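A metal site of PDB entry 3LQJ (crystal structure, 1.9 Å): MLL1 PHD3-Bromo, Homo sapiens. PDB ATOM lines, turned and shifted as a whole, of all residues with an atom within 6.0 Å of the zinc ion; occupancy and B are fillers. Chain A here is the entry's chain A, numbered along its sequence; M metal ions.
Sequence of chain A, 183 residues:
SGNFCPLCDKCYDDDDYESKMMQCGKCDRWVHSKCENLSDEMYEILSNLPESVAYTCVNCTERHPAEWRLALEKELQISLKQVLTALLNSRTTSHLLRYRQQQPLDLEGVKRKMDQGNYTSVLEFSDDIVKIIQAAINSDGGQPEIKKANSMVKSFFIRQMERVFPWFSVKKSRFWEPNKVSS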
ATOM      1  N   CYS A  24      11.149  -1.897  -1.944  1.00  0.00           N
ATOM      2  CA  CYS A  24      10.313  -0.902  -1.297  1.00  0.00           C
ATOM      3  C   CYS A  24      10.610  -0.924   0.204  1.00  0.00           C
ATOM      4  O   CYS A  24      10.553  -1.975   0.836  1.00  0.00           O
ATOM      5  CB  CYS A  24       8.828  -1.201  -1.535  1.00  0.00           C
ATOM      6  SG  CYS A  24       7.741  -0.120  -0.562  1.00  0.00           S
ATOM      7  N   GLY A  25      10.931   0.236   0.763  1.00  0.00           N
ATOM      8  CA  GLY A  25      11.244   0.289   2.180  1.00  0.00           C
ATOM      9  C   GLY A  25      10.038   0.077   3.098  1.00  0.00           C
ATOM     10  O   GLY A  25      10.192  -0.029   4.314  1.00  0.00           O
ATOM     11  N   LYS A  26       8.843   0.019   2.509  1.00  0.00           N
ATOM     12  CA  LYS A  26       7.623  -0.162   3.279  1.00  0.00           C
ATOM     13  C   LYS A  26       7.161  -1.618   3.367  1.00  0.00           C
ATOM     14  O   LYS A  26       7.006  -2.156   4.465  1.00  0.00           O
ATOM     15  CB  LYS A  26       6.493   0.690   2.681  1.00  0.00           C
ATOM     16  CG  LYS A  26       6.640   2.193   2.879  1.00  0.00           C
ATOM     17  CD  LYS A  26       6.238   2.613   4.286  1.00  0.00           C
ATOM     18  CE  LYS A  26       6.593   4.066   4.566  1.00  0.00           C
ATOM     19  NZ  LYS A  26       5.967   5.012   3.604  1.00  0.00           N
ATOM     20  N   CYS A  27       6.944  -2.257   2.220  1.00  0.00           N
ATOM     21  CA  CYS A  27       6.466  -3.632   2.177  1.00  0.00           C
ATOM     22  C   CYS A  27       7.544  -4.680   1.873  1.00  0.00           C
ATOM     23  O   CYS A  27       7.266  -5.883   1.916  1.00  0.00           O
ATOM     24  CB  CYS A  27       5.339  -3.759   1.148  1.00  0.00           C
ATOM     25  SG  CYS A  27       5.886  -3.522  -0.562  1.00  0.00           S
ATOM     26  N   ASP A  28       8.746  -4.230   1.550  1.00  0.00           N
ATOM     27  CA  ASP A  28       9.857  -5.139   1.242  1.00  0.00           C
ATOM     28  C   ASP A  28       9.799  -5.856  -0.114  1.00  0.00           C
ATOM     29  O   ASP A  28      10.627  -6.725  -0.374  1.00  0.00           O
ATOM     30  CB  ASP A  28      10.040  -6.186   2.345  1.00  0.00           C
ATOM     31  CG  ASP A  28      10.393  -5.577   3.691  1.00  0.00           C
ATOM     32  OD1 ASP A  28      11.055  -4.520   3.708  1.00  0.00           O
ATOM     33  OD2 ASP A  28      10.035  -6.174   4.727  1.00  0.00           O
ATOM     34  N   ARG A  29       8.851  -5.516  -0.971  1.00  0.00           N
ATOM     35  CA  ARG A  29       8.802  -6.199  -2.267  1.00  0.00           C
ATOM     36  C   ARG A  29       9.790  -5.574  -3.241  1.00  0.00           C
ATOM     37  O   ARG A  29      10.231  -4.442  -3.066  1.00  0.00           O
ATOM     38  CB  ARG A  29       7.396  -6.172  -2.858  1.00  0.00           C
ATOM     39  CG  ARG A  29       7.002  -4.860  -3.508  1.00  0.00           C
ATOM     40  CD  ARG A  29       5.553  -4.945  -3.988  1.00  0.00           C
ATOM     41  NE  ARG A  29       5.314  -6.089  -4.879  1.00  0.00           N
ATOM     42  CZ  ARG A  29       4.114  -6.400  -5.349  1.00  0.00           C
ATOM     43  NH1 ARG A  29       3.068  -5.671  -5.018  1.00  0.00           N
ATOM     44  NH2 ARG A  29       3.953  -7.440  -6.163  1.00  0.00           N
ATOM     45  N   THR A  56      10.255   3.434  -2.786  1.00  0.00           N
ATOM     46  CA  THR A  56       8.912   3.114  -2.355  1.00  0.00           C
ATOM     47  C   THR A  56       8.084   2.725  -3.588  1.00  0.00           C
ATOM     48  O   THR A  56       8.069   3.454  -4.577  1.00  0.00           O
ATOM     49  CB  THR A  56       8.352   4.350  -1.583  1.00  0.00           C
ATOM     50  OG1 THR A  56       7.740   3.912  -0.370  1.00  0.00           O
ATOM     51  CG2 THR A  56       7.374   5.124  -2.413  1.00  0.00           C
ATOM     52  N   CYS A  57       7.432   1.561  -3.554  1.00  0.00           N
ATOM     53  CA  CYS A  57       6.615   1.118  -4.690  1.00  0.00           C
ATOM     54  C   CYS A  57       5.372   1.982  -4.831  1.00  0.00           C
ATOM     55  O   CYS A  57       4.977   2.673  -3.890  1.00  0.00           O
ATOM     56  CB  CYS A  57       6.224  -0.367  -4.547  1.00  0.00           C
ATOM     57  SG  CYS A  57       4.965  -0.756  -3.291  1.00  0.00           S
ATOM     58  N   VAL A  58       4.750   1.953  -6.000  1.00  0.00           N
ATOM     59  CA  VAL A  58       3.570   2.777  -6.269  1.00  0.00           C
ATOM     60  C   VAL A  58       2.464   2.771  -5.216  1.00  0.00           C
ATOM     61  O   VAL A  58       2.096   3.817  -4.681  1.00  0.00           O
ATOM     62  CB  VAL A  58       2.915   2.416  -7.615  1.00  0.00           C
ATOM     63  CG1 VAL A  58       1.591   3.161  -7.773  1.00  0.00           C
ATOM     64  CG2 VAL A  58       3.848   2.781  -8.755  1.00  0.00           C
ATOM     65  N   ASN A  59       1.926   1.591  -4.916  1.00  0.00           N
ATOM     66  CA  ASN A  59       0.834   1.500  -3.946  1.00  0.00           C
ATOM     67  C   ASN A  59       1.244   1.881  -2.533  1.00  0.00           C
ATOM     68  O   ASN A  59       0.406   2.323  -1.747  1.00  0.00           O
ATOM     69  CB  ASN A  59       0.225   0.109  -3.991  1.00  0.00           C
ATOM     70  CG  ASN A  59      -0.280  -0.248  -5.382  1.00  0.00           C
ATOM     71  OD1 ASN A  59      -1.080   0.487  -5.963  1.00  0.00           O
ATOM     72  ND2 ASN A  59       0.188  -1.356  -5.914  1.00  0.00           N
ATOM     73  N   CYS A  60       2.513   1.720  -2.202  1.00  0.00           N
ATOM     74  CA  CYS A  60       2.990   2.103  -0.879  1.00  0.00           C
ATOM     75  C   CYS A  60       3.290   3.601  -0.856  1.00  0.00           C
ATOM     76  O   CYS A  60       3.532   4.174   0.208  1.00  0.00           O
ATOM     77  CB  CYS A  60       4.252   1.325  -0.496  1.00  0.00           C
ATOM     78  SG  CYS A  60       3.915  -0.250   0.294  1.00  0.00           S
HETATM   79 ZN    ZN M   1       5.665  -1.247  -1.135  1.00  0.00          ZN
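SG of Cys 27 lies close to N of Arg 29 (3.6 Å). The side-chain sulfur (SG) of Cys 24 sits close to the backbone NH (N) of Lys 26, 3.3 Å away. N of Cys 24 lies within hydrogen-bond range of O of Arg 29 (2.9 Å).
Within 4 Å of the zinc ion: Cys 24, Cys 27, Cys 57 and Cys 60. Along chain A the residues within 4 Å of the zinc ion span positions 24 to 60.
The zinc ion is bound by the side-chain sulfur of Cys 57 (2.3 Å), the side-chain sulfur of Cys 27 (2.4 Å), the side-chain sulfur of Cys 24 (2.4 Å) and the side-chain sulfur of Cys 60 (2.5 Å).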
